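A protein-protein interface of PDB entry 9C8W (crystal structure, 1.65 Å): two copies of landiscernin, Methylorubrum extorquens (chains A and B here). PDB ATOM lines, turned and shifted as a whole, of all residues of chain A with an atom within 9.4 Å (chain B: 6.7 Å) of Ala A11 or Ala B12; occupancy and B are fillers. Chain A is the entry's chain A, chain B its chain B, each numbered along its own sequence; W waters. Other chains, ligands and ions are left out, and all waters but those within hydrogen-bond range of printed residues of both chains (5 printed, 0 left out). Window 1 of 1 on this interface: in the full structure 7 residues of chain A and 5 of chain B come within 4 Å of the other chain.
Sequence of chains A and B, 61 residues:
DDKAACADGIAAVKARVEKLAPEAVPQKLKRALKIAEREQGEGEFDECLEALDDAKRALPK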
ATOM      1  N   LYS A   3       5.250  35.950  16.729  1.00  0.00           N
ATOM      2  CA  LYS A   3       5.108  35.401  15.381  1.00  0.00           C
ATOM      3  C   LYS A   3       6.126  34.295  15.134  1.00  0.00           C
ATOM      4  O   LYS A   3       5.779  33.212  14.643  1.00  0.00           O
ATOM      5  CB  LYS A   3       5.270  36.516  14.338  1.00  0.00           C
ATOM      6  CG  LYS A   3       5.447  36.020  12.898  1.00  0.00           C
ATOM      7  CD  LYS A   3       5.404  37.183  11.907  1.00  0.00           C
ATOM      8  CE  LYS A   3       5.921  36.802  10.521  1.00  0.00           C
ATOM      9  NZ  LYS A   3       4.991  35.980   9.705  1.00  0.00           N
ATOM     10  N   ALA A   4       7.391  34.542  15.504  1.00  0.00           N
ATOM     11  CA  ALA A   4       8.430  33.539  15.299  1.00  0.00           C
ATOM     12  C   ALA A   4       8.253  32.348  16.236  1.00  0.00           C
ATOM     13  O   ALA A   4       8.426  31.196  15.819  1.00  0.00           O
ATOM     14  CB  ALA A   4       9.809  34.175  15.492  1.00  0.00           C
ATOM     15  N   ALA A   5       7.890  32.600  17.497  1.00  0.00           N
ATOM     16  CA  ALA A   5       7.680  31.497  18.432  1.00  0.00           C
ATOM     17  C   ALA A   5       6.508  30.628  18.006  1.00  0.00           C
ATOM     18  O   ALA A   5       6.525  29.408  18.230  1.00  0.00           O
ATOM     19  CB  ALA A   5       7.455  32.025  19.849  1.00  0.00           C
ATOM     20  N   CYS A   6       5.483  31.230  17.399  1.00  0.00           N
ATOM     21  CA  CYS A   6       4.336  30.452  16.929  1.00  0.00           C
ATOM     22  C   CYS A   6       4.732  29.524  15.783  1.00  0.00           C
ATOM     23  O   CYS A   6       4.420  28.329  15.808  1.00  0.00           O
ATOM     24  CB  CYS A   6       3.200  31.394  16.524  1.00  0.00           C
ATOM     25  SG  CYS A   6       1.815  30.591  15.663  1.00  0.00           S
ATOM     26  N   ALA A   7       5.461  30.041  14.788  1.00  0.00           N
ATOM     27  CA  ALA A   7       5.895  29.192  13.680  1.00  0.00           C
ATOM     28  C   ALA A   7       6.858  28.110  14.150  1.00  0.00           C
ATOM     29  O   ALA A   7       6.735  26.937  13.756  1.00  0.00           O
ATOM     30  CB  ALA A   7       6.551  30.044  12.590  1.00  0.00           C
ATOM     31  N   ASP A   8       7.830  28.492  14.989  1.00  0.00           N
ATOM     32  CA  ASP A   8       8.803  27.534  15.508  1.00  0.00           C
ATOM     33  C   ASP A   8       8.122  26.447  16.326  1.00  0.00           C
ATOM     34  O   ASP A   8       8.523  25.276  16.281  1.00  0.00           O
ATOM     35  CB  ASP A   8       9.837  28.257  16.369  1.00  0.00           C
ATOM     36  CG  ASP A   8      10.780  29.140  15.560  1.00  0.00           C
ATOM     37  OD1 ASP A   8      10.723  29.157  14.307  1.00  0.00           O
ATOM     38  OD2 ASP A   8      11.580  29.858  16.198  1.00  0.00           O
ATOM     39  N   GLY A   9       7.119  26.829  17.119  1.00  0.00           N
ATOM     40  CA  GLY A   9       6.446  25.852  17.963  1.00  0.00           C
ATOM     41  C   GLY A   9       5.595  24.885  17.165  1.00  0.00           C
ATOM     42  O   GLY A   9       5.522  23.697  17.483  1.00  0.00           O
ATOM     43  N   ILE A  10       4.930  25.379  16.121  1.00  0.00           N
ATOM     44  CA  ILE A  10       4.179  24.489  15.243  1.00  0.00           C
ATOM     45  C   ILE A  10       5.127  23.512  14.574  1.00  0.00           C
ATOM     46  O   ILE A  10       4.861  22.305  14.511  1.00  0.00           O
ATOM     47  CB  ILE A  10       3.391  25.303  14.203  1.00  0.00           C
ATOM     48  CG1 ILE A  10       2.220  26.028  14.876  1.00  0.00           C
ATOM     49  CG2 ILE A  10       2.870  24.386  13.088  1.00  0.00           C
ATOM     50  CD1 ILE A  10       1.539  27.047  13.942  1.00  0.00           C
ATOM     51  N   ALA A  11       6.272  24.011  14.102  1.00  0.00           N
ATOM     52  CA  ALA A  11       7.250  23.117  13.494  1.00  0.00           C
ATOM     53  C   ALA A  11       7.741  22.072  14.491  1.00  0.00           C
ATOM     54  O   ALA A  11       7.894  20.893  14.147  1.00  0.00           O
ATOM     55  CB  ALA A  11       8.426  23.923  12.941  1.00  0.00           C
ATOM     56  N   ALA A  12       7.980  22.484  15.736  1.00  0.00           N
ATOM     57  CA  ALA A  12       8.502  21.557  16.737  1.00  0.00           C
ATOM     58  C   ALA A  12       7.475  20.489  17.096  1.00  0.00           C
ATOM     59  O   ALA A  12       7.820  19.306  17.228  1.00  0.00           O
ATOM     60  CB  ALA A  12       8.943  22.323  17.983  1.00  0.00           C
ATOM     61  N   VAL A  13       6.215  20.882  17.276  1.00  0.00           N
ATOM     62  CA  VAL A  13       5.194  19.891  17.604  1.00  0.00           C
ATOM     63  C   VAL A  13       4.998  18.917  16.446  1.00  0.00           C
ATOM     64  O   VAL A  13       4.900  17.703  16.654  1.00  0.00           O
ATOM     65  CB  VAL A  13       3.875  20.582  17.990  1.00  0.00           C
ATOM     66  CG1 VAL A  13       2.760  19.536  18.168  1.00  0.00           C
ATOM     67  CG2 VAL A  13       4.057  21.401  19.256  1.00  0.00           C
ATOM     68  N   LYS A  14       4.959  19.427  15.208  1.00  0.00           N
ATOM     69  CA  LYS A  14       4.795  18.550  14.055  1.00  0.00           C
ATOM     70  C   LYS A  14       5.912  17.512  13.974  1.00  0.00           C
ATOM     71  O   LYS A  14       5.650  16.350  13.648  1.00  0.00           O
ATOM     72  CB  LYS A  14       4.720  19.372  12.768  1.00  0.00           C
ATOM     73  CG  LYS A  14       3.373  20.037  12.567  1.00  0.00           C
ATOM     74  CD  LYS A  14       3.319  20.801  11.268  1.00  0.00           C
ATOM     75  CE  LYS A  14       1.893  20.975  10.837  1.00  0.00           C
ATOM     76  NZ  LYS A  14       1.787  21.740   9.569  1.00  0.00           N
ATOM     77  N   ALA A  15       7.165  17.911  14.254  1.00  0.00           N
ATOM     78  CA  ALA A  15       8.272  16.955  14.207  1.00  0.00           C
ATOM     79  C   ALA A  15       8.168  15.918  15.323  1.00  0.00           C
ATOM     80  O   ALA A  15       8.505  14.747  15.118  1.00  0.00           O
ATOM     81  CB  ALA A  15       9.619  17.677  14.267  1.00  0.00           C
ATOM     82  N   ARG A  16       7.737  16.334  16.517  1.00  0.00           N
ATOM     83  CA  ARG A  16       7.511  15.369  17.589  1.00  0.00           C
ATOM     84  C   ARG A  16       6.401  14.386  17.218  1.00  0.00           C
ATOM     85  O   ARG A  16       6.528  13.182  17.463  1.00  0.00           O
ATOM     86  CB  ARG A  16       7.163  16.086  18.899  1.00  0.00           C
ATOM     87  CG  ARG A  16       8.247  16.988  19.517  1.00  0.00           C
ATOM     88  CD  ARG A  16       7.791  17.420  20.915  1.00  0.00           C
ATOM     89  NE  ARG A  16       8.676  18.353  21.605  1.00  0.00           N
ATOM     90  CZ  ARG A  16       8.429  18.867  22.808  1.00  0.00           C
ATOM     91  NH1 ARG A  16       7.345  18.534  23.497  1.00  0.00           N
ATOM     92  NH2 ARG A  16       9.276  19.754  23.324  1.00  0.00           N
ATOM     93  N   VAL A  17       5.301  14.883  16.638  1.00  0.00           N
ATOM     94  CA  VAL A  17       4.180  14.016  16.259  1.00  0.00           C
ATOM     95  C   VAL A  17       4.605  12.998  15.212  1.00  0.00           C
ATOM     96  O   VAL A  17       4.176  11.838  15.243  1.00  0.00           O
ATOM     97  CB  VAL A  17       2.989  14.868  15.773  1.00  0.00           C
ATOM     98  CG1 VAL A  17       1.947  14.004  15.070  1.00  0.00           C
ATOM     99  CG2 VAL A  17       2.355  15.568  16.948  1.00  0.00           C
ATOM    100  N   GLU A  18       5.483  13.399  14.288  1.00  0.00           N
ATOM    101  CA  GLU A  18       5.909  12.484  13.234  1.00  0.00           C
ATOM    102  C   GLU A  18       6.664  11.290  13.800  1.00  0.00           C
ATOM    103  O   GLU A  18       6.722  10.238  13.160  1.00  0.00           O
ATOM    104  CB  GLU A  18       6.779  13.217  12.214  1.00  0.00           C
ATOM    105  CG  GLU A  18       7.096  12.391  10.990  1.00  0.00           C
ATOM    106  CD  GLU A  18       8.100  13.059  10.071  1.00  0.00           C
ATOM    107  OE1 GLU A  18       8.353  14.272  10.240  1.00  0.00           O
ATOM    108  OE2 GLU A  18       8.649  12.362   9.187  1.00  0.00           O
ATOM    109  N   LEU A  33      -3.328  21.505  18.033  1.00  0.00           N
ATOM    110  CA  LEU A  33      -2.464  21.889  16.924  1.00  0.00           C
ATOM    111  C   LEU A  33      -3.272  22.557  15.820  1.00  0.00           C
ATOM    112  O   LEU A  33      -2.815  23.536  15.225  1.00  0.00           O
ATOM    113  CB  LEU A  33      -1.704  20.673  16.385  1.00  0.00           C
ATOM    114  CG  LEU A  33      -0.721  20.927  15.234  1.00  0.00           C
ATOM    115  CD1 LEU A  33       0.380  21.887  15.662  1.00  0.00           C
ATOM    116  CD2 LEU A  33      -0.136  19.613  14.729  1.00  0.00           C
ATOM    117  N   ALA A  36      -3.880  26.104  16.889  1.00  0.00           N
ATOM    118  CA  ALA A  36      -2.665  26.903  16.743  1.00  0.00           C
ATOM    119  C   ALA A  36      -2.461  27.334  15.292  1.00  0.00           C
ATOM    120  O   ALA A  36      -2.153  28.503  15.018  1.00  0.00           O
ATOM    121  CB  ALA A  36      -1.454  26.109  17.248  1.00  0.00           C
ATOM    122  N   GLU A  37      -2.640  26.402  14.349  1.00  0.00           N
ATOM    123  CA  GLU A  37      -2.439  26.722  12.937  1.00  0.00           C
ATOM    124  C   GLU A  37      -3.481  27.710  12.438  1.00  0.00           C
ATOM    125  O   GLU A  37      -3.169  28.580  11.616  1.00  0.00           O
ATOM    126  CB  GLU A  37      -2.484  25.447  12.089  1.00  0.00           C
ATOM    127  CG  GLU A  37      -1.317  24.505  12.283  1.00  0.00           C
ATOM    128  CD  GLU A  37      -1.599  23.134  11.681  1.00  0.00           C
ATOM    129  OE1 GLU A  37      -2.782  22.789  11.513  1.00  0.00           O
ATOM    130  OE2 GLU A  37      -0.647  22.397  11.403  1.00  0.00           O
ATOM    131  N   GLN A  40      -2.483  31.051  13.862  1.00  0.00           N
ATOM    132  CA  GLN A  40      -1.334  31.578  13.128  1.00  0.00           C
ATOM    133  C   GLN A  40      -1.768  32.228  11.825  1.00  0.00           C
ATOM    134  O   GLN A  40      -1.317  33.334  11.489  1.00  0.00           O
ATOM    135  CB  GLN A  40      -0.321  30.469  12.842  1.00  0.00           C
ATOM    136  CG  GLN A  40       0.851  30.951  11.965  1.00  0.00           C
ATOM    137  CD  GLN A  40       1.701  29.819  11.464  1.00  0.00           C
ATOM    138  OE1 GLN A  40       1.188  28.845  10.906  1.00  0.00           O
ATOM    139  NE2 GLN A  40       3.009  29.936  11.644  1.00  0.00           N
ATOM    140  N   CYS A  48      -1.906  31.508  19.463  1.00  0.00           N
ATOM    141  CA  CYS A  48      -1.229  30.323  18.932  1.00  0.00           C
ATOM    142  C   CYS A  48      -0.298  29.707  19.969  1.00  0.00           C
ATOM    143  O   CYS A  48      -0.240  28.479  20.105  1.00  0.00           O
ATOM    144  CB  CYS A  48      -0.462  30.688  17.654  1.00  0.00           C
ATOM    145  SG  CYS A  48       0.802  29.486  17.102  1.00  0.00           S
ATOM    146  N   LEU A  52      -0.367  25.954  21.465  1.00  0.00           N
ATOM    147  CA  LEU A  52       0.808  25.086  21.405  1.00  0.00           C
ATOM    148  C   LEU A  52       1.177  24.543  22.778  1.00  0.00           C
ATOM    149  O   LEU A  52       1.657  23.410  22.884  1.00  0.00           O
ATOM    150  CB  LEU A  52       2.001  25.837  20.812  1.00  0.00           C
ATOM    151  CG  LEU A  52       1.962  26.073  19.300  1.00  0.00           C
ATOM    152  CD1 LEU A  52       3.064  27.047  18.865  1.00  0.00           C
ATOM    153  CD2 LEU A  52       2.112  24.758  18.558  1.00  0.00           C
ATOM    154  N   LYS A  56       1.607  20.518  23.476  1.00  0.00           N
ATOM    155  CA  LYS A  56       2.779  19.861  24.044  1.00  0.00           C
ATOM    156  C   LYS A  56       2.445  19.153  25.351  1.00  0.00           C
ATOM    157  O   LYS A  56       2.997  18.082  25.637  1.00  0.00           O
ATOM    158  CB  LYS A  56       3.888  20.887  24.276  1.00  0.00           C
ATOM    159  CG  LYS A  56       4.501  21.449  23.000  1.00  0.00           C
ATOM    160  CD  LYS A  56       5.654  22.387  23.338  1.00  0.00           C
ATOM    161  CE  LYS A  56       5.187  23.648  24.012  1.00  0.00           C
ATOM    162  NZ  LYS A  56       6.356  24.552  24.258  1.00  0.00           N
ATOM    163  N   LEU A  59       1.331  15.525  24.638  1.00  0.00           N
ATOM    164  CA  LEU A  59       2.261  14.549  24.091  1.00  0.00           C
ATOM    165  C   LEU A  59       2.662  13.517  25.148  1.00  0.00           C
ATOM    166  O   LEU A  59       2.773  13.838  26.336  1.00  0.00           O
ATOM    167  CB  LEU A  59       3.500  15.246  23.549  1.00  0.00           C
ATOM    168  CG  LEU A  59       3.227  16.048  22.273  1.00  0.00           C
ATOM    169  CD1 LEU A  59       4.456  16.808  21.851  1.00  0.00           C
ATOM    170  CD2 LEU A  59       2.752  15.119  21.158  1.00  0.00           C
ATOM    171  N   ALA B   7      16.321  19.727  20.122  1.00  0.00           N
ATOM    172  CA  ALA B   7      15.568  19.039  19.078  1.00  0.00           C
ATOM    173  C   ALA B   7      14.477  19.935  18.502  1.00  0.00           C
ATOM    174  O   ALA B   7      14.302  19.999  17.281  1.00  0.00           O
ATOM    175  CB  ALA B   7      14.965  17.745  19.624  1.00  0.00           C
ATOM    176  N   ASP B   8      13.731  20.633  19.364  1.00  0.00           N
ATOM    177  CA  ASP B   8      12.692  21.537  18.871  1.00  0.00           C
ATOM    178  C   ASP B   8      13.282  22.645  18.012  1.00  0.00           C
ATOM    179  O   ASP B   8      12.687  23.042  17.005  1.00  0.00           O
ATOM    180  CB  ASP B   8      11.921  22.157  20.038  1.00  0.00           C
ATOM    181  CG  ASP B   8      11.008  21.174  20.729  1.00  0.00           C
ATOM    182  OD1 ASP B   8      10.891  20.003  20.265  1.00  0.00           O
ATOM    183  OD2 ASP B   8      10.402  21.591  21.747  1.00  0.00           O
ATOM    184  N   GLY B   9      14.434  23.180  18.420  1.00  0.00           N
ATOM    185  CA  GLY B   9      15.041  24.273  17.678  1.00  0.00           C
ATOM    186  C   GLY B   9      15.578  23.828  16.334  1.00  0.00           C
ATOM    187  O   GLY B   9      15.509  24.573  15.355  1.00  0.00           O
ATOM    188  N   ILE B  10      16.145  22.621  16.275  1.00  0.00           N
ATOM    189  CA  ILE B  10      16.572  22.081  14.988  1.00  0.00           C
ATOM    190  C   ILE B  10      15.368  21.905  14.071  1.00  0.00           C
ATOM    191  O   ILE B  10      15.418  22.255  12.885  1.00  0.00           O
ATOM    192  CB  ILE B  10      17.351  20.770  15.193  1.00  0.00           C
ATOM    193  CG1 ILE B  10      18.714  21.095  15.805  1.00  0.00           C
ATOM    194  CG2 ILE B  10      17.505  20.021  13.873  1.00  0.00           C
ATOM    195  CD1 ILE B  10      19.499  19.891  16.260  1.00  0.00           C
ATOM    196  N   ALA B  11      14.258  21.390  14.608  1.00  0.00           N
ATOM    197  CA  ALA B  11      13.043  21.282  13.804  1.00  0.00           C
ATOM    198  C   ALA B  11      12.573  22.653  13.328  1.00  0.00           C
ATOM    199  O   ALA B  11      12.169  22.816  12.167  1.00  0.00           O
ATOM    200  CB  ALA B  11      11.938  20.587  14.609  1.00  0.00           C
ATOM    201  N   ALA B  12      12.634  23.657  14.206  1.00  0.00           N
ATOM    202  CA  ALA B  12      12.160  24.984  13.832  1.00  0.00           C
ATOM    203  C   ALA B  12      13.041  25.594  12.749  1.00  0.00           C
ATOM    204  O   ALA B  12      12.531  26.161  11.780  1.00  0.00           O
ATOM    205  CB  ALA B  12      12.108  25.895  15.065  1.00  0.00           C
ATOM    206  N   VAL B  13      14.361  25.481  12.890  1.00  0.00           N
ATOM    207  CA  VAL B  13      15.252  26.044  11.877  1.00  0.00           C
ATOM    208  C   VAL B  13      15.089  25.310  10.551  1.00  0.00           C
ATOM    209  O   VAL B  13      15.029  25.937   9.486  1.00  0.00           O
ATOM    210  CB  VAL B  13      16.710  26.017  12.371  1.00  0.00           C
ATOM    211  CG1 VAL B  13      17.651  26.435  11.256  1.00  0.00           C
ATOM    212  CG2 VAL B  13      16.871  26.928  13.574  1.00  0.00           C
ATOM    213  N   LYS B  14      14.993  23.977  10.591  1.00  0.00           N
ATOM    214  CA  LYS B  14      14.815  23.209   9.359  1.00  0.00           C
ATOM    215  C   LYS B  14      13.550  23.631   8.619  1.00  0.00           C
ATOM    216  O   LYS B  14      13.541  23.714   7.385  1.00  0.00           O
ATOM    217  CB  LYS B  14      14.768  21.709   9.669  1.00  0.00           C
ATOM    218  CG  LYS B  14      16.135  21.088   9.963  1.00  0.00           C
ATOM    219  CD  LYS B  14      16.032  19.585  10.212  1.00  0.00           C
ATOM    220  CE  LYS B  14      16.658  18.790   9.082  1.00  0.00           C
ATOM    221  NZ  LYS B  14      16.011  19.108   7.775  1.00  0.00           N
ATOM    222  N   ALA B  15      12.470  23.902   9.362  1.00  0.00           N
ATOM    223  CA  ALA B  15      11.212  24.303   8.746  1.00  0.00           C
ATOM    224  C   ALA B  15      11.345  25.640   8.034  1.00  0.00           C
ATOM    225  O   ALA B  15      10.790  25.830   6.943  1.00  0.00           O
ATOM    226  CB  ALA B  15      10.120  24.387   9.811  1.00  0.00           C
ATOM    227  N   ARG B  16      12.084  26.574   8.635  1.00  0.00           N
ATOM    228  CA  ARG B  16      12.336  27.851   7.978  1.00  0.00           C
ATOM    229  C   ARG B  16      13.153  27.664   6.712  1.00  0.00           C
ATOM    230  O   ARG B  16      12.843  28.244   5.667  1.00  0.00           O
ATOM    231  CB  ARG B  16      13.045  28.786   8.955  1.00  0.00           C
ATOM    232  CG  ARG B  16      12.163  29.144  10.125  1.00  0.00           C
ATOM    233  CD  ARG B  16      12.766  30.204  10.991  1.00  0.00           C
ATOM    234  NE  ARG B  16      11.845  30.549  12.063  1.00  0.00           N
ATOM    235  CZ  ARG B  16      10.954  31.523  11.966  1.00  0.00           C
ATOM    236  NH1 ARG B  16      10.866  32.273  10.874  1.00  0.00           N
ATOM    237  NH2 ARG B  16      10.110  31.734  12.971  1.00  0.00           N
ATOM    238  N   VAL B  17      14.191  26.832   6.783  1.00  0.00           N
ATOM    239  CA  VAL B  17      15.050  26.616   5.626  1.00  0.00           C
ATOM    240  C   VAL B  17      14.274  25.987   4.474  1.00  0.00           C
ATOM    241  O   VAL B  17      14.526  26.300   3.303  1.00  0.00           O
ATOM    242  CB  VAL B  17      16.267  25.770   6.045  1.00  0.00           C
ATOM    243  CG1 VAL B  17      17.059  25.295   4.828  1.00  0.00           C
ATOM    244  CG2 VAL B  17      17.148  26.578   6.992  1.00  0.00           C
ATOM    245  N   LYS B  56      19.250  31.639  13.879  1.00  0.00           N
ATOM    246  CA  LYS B  56      18.087  32.519  13.852  1.00  0.00           C
ATOM    247  C   LYS B  56      18.474  33.973  13.595  1.00  0.00           C
ATOM    248  O   LYS B  56      17.657  34.743  13.076  1.00  0.00           O
ATOM    249  CB  LYS B  56      17.287  32.358  15.143  1.00  0.00           C
ATOM    250  CG  LYS B  56      16.583  31.003  15.191  1.00  0.00           C
ATOM    251  CD  LYS B  56      15.718  30.799  16.426  1.00  0.00           C
ATOM    252  CE  LYS B  56      16.540  30.660  17.688  1.00  0.00           C
ATOM    253  NZ  LYS B  56      15.654  30.360  18.851  1.00  0.00           N
HETATM  254  O   HOH W   1      10.014  27.292  12.250  1.00  0.00           O
HETATM  255  O   HOH W   2      13.447  28.369  17.741  1.00  0.00           O
HETATM  256  O   HOH W   3      11.608  17.478  21.613  1.00  0.00           O
HETATM  257  O   HOH W   4      10.593  18.895  17.756  1.00  0.00           O
HETATM  258  O   HOH W   5      12.980  31.814  15.005  1.00  0.00           O
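Water W5 lies within hydrogen-bond range of OD2 of Asp A8 (2.7 Å) and NE of Arg B16 (3.4 Å).
Water W4 bridges OD1 of Asp B8 and O of Ala A12.
Water W1 bridges O of Ala B12 (2.8 Å) and OD1 of Asp A8 (2.9 Å).
Water W2 lies within hydrogen-bond range of the side-chain carboxylate of Asp A8 and the side-chain amino group of Lys B56.
Water W3 lies within hydrogen-bond range of OD1 of Asp B8 (3.0 Å) and NE of Arg A16 (3.1 Å).
No residue of chain A comes within 4 Å of Gly B9.
Ala B11 touches just these residues of chain A: Ala A11 (3.98 Å) and Ala A15 (3.7 Å).
No residue of chain A comes within 4 Å of Val B13.
Of chain A, only Ala A11 (3.6 Å) comes within 4 Å of Ala B15.
Printed residues of chain A within 4 Å of Arg B16: Ala A4 (3.4 Å), Ala A7 (3.96 Å) and Asp A8 (2.9 Å).
Of the printed residues of chain B, Arg A16 touches Asp B8 (2.7 Å).
Printed residues of chain B within 4 Å of Ala A7: Arg B16.
Of the printed residues of chain A, Asp B8 touches Ala A12 and Arg A16.
Printed residues of chain B within 4 Å of Ala A4: Arg B16.
The nearest printed residue of chain B that does not touch Ala A11 is Asp B8 (5.6 Å).
Asp A8 touches Ala B12, and with the chains exchanged Ala A12 touches Asp B8.
Ala B11 touches its own counterpart, Ala A11.
Ala A11 touches Ala B12, but with the chains exchanged Ala A12 does not touch Ala B11 (4.2 Å).
Ala A11 touches Ala B15, and with the chains exchanged Ala A15 touches Ala B11.
Positions printed for both chains: 7, 8, 9, 10, 11, 12, 13, 14, 15, 16, 17 and 56.
Of the 10 pairs that touch across the chains among the printed residues, 7 have their exchanged pair printed and touching as well.
The guanidinium group (NH2) of Arg B16 lies within hydrogen-bond range of the backbone carbonyl oxygen (O) of Ala A4, 3.4 Å away.
The side-chain carboxylate (OD1) of Asp A8 lies within salt-bridge range of the guanidinium group (NE) of Arg B16 (2.9 Å).
The side-chain carboxylate (OD2) of Asp B8 is in salt-bridge range of the guanidinium group (NH2) of Arg A16 (2.7 Å).
Of the 24 printed residues of chain A, 7 touch a printed residue of chain B.
Hydrophobic or aromatic side chains of chain A that line the printed part of chain B: Ala A4, Ala A7, Ala A11, Ala A12 and Ala A15.
Along chain A the printed residues that touch a printed residue of chain B span positions 4 to 16.
Hydrophobic or aromatic side chains of chain B that line the printed part of chain A: Ala B11, Ala B12 and Ala B15.
Along chain B the printed residues that touch a printed residue of chain A span positions 8 to 16.
Among the printed residues, 10 pairs touch across the chains.
Among the printed residues, merely in contact across the chains: Asp A8 with Ala B12 (3.5 Å), Ala A11 with Ala B15 (3.6 Å), Ala A12 with Asp B8 (3.6 Å), Ala A15 with Ala B11 (3.7 Å), Ala A7 with Arg B16 (3.96 Å), Ala A11 with Ala B11 (3.98 Å) and Ala A11 with Ala B12 (3.98 Å).
SG of Cys A6 forms a disulfide with SG of Cys A48 (2.1 Å).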
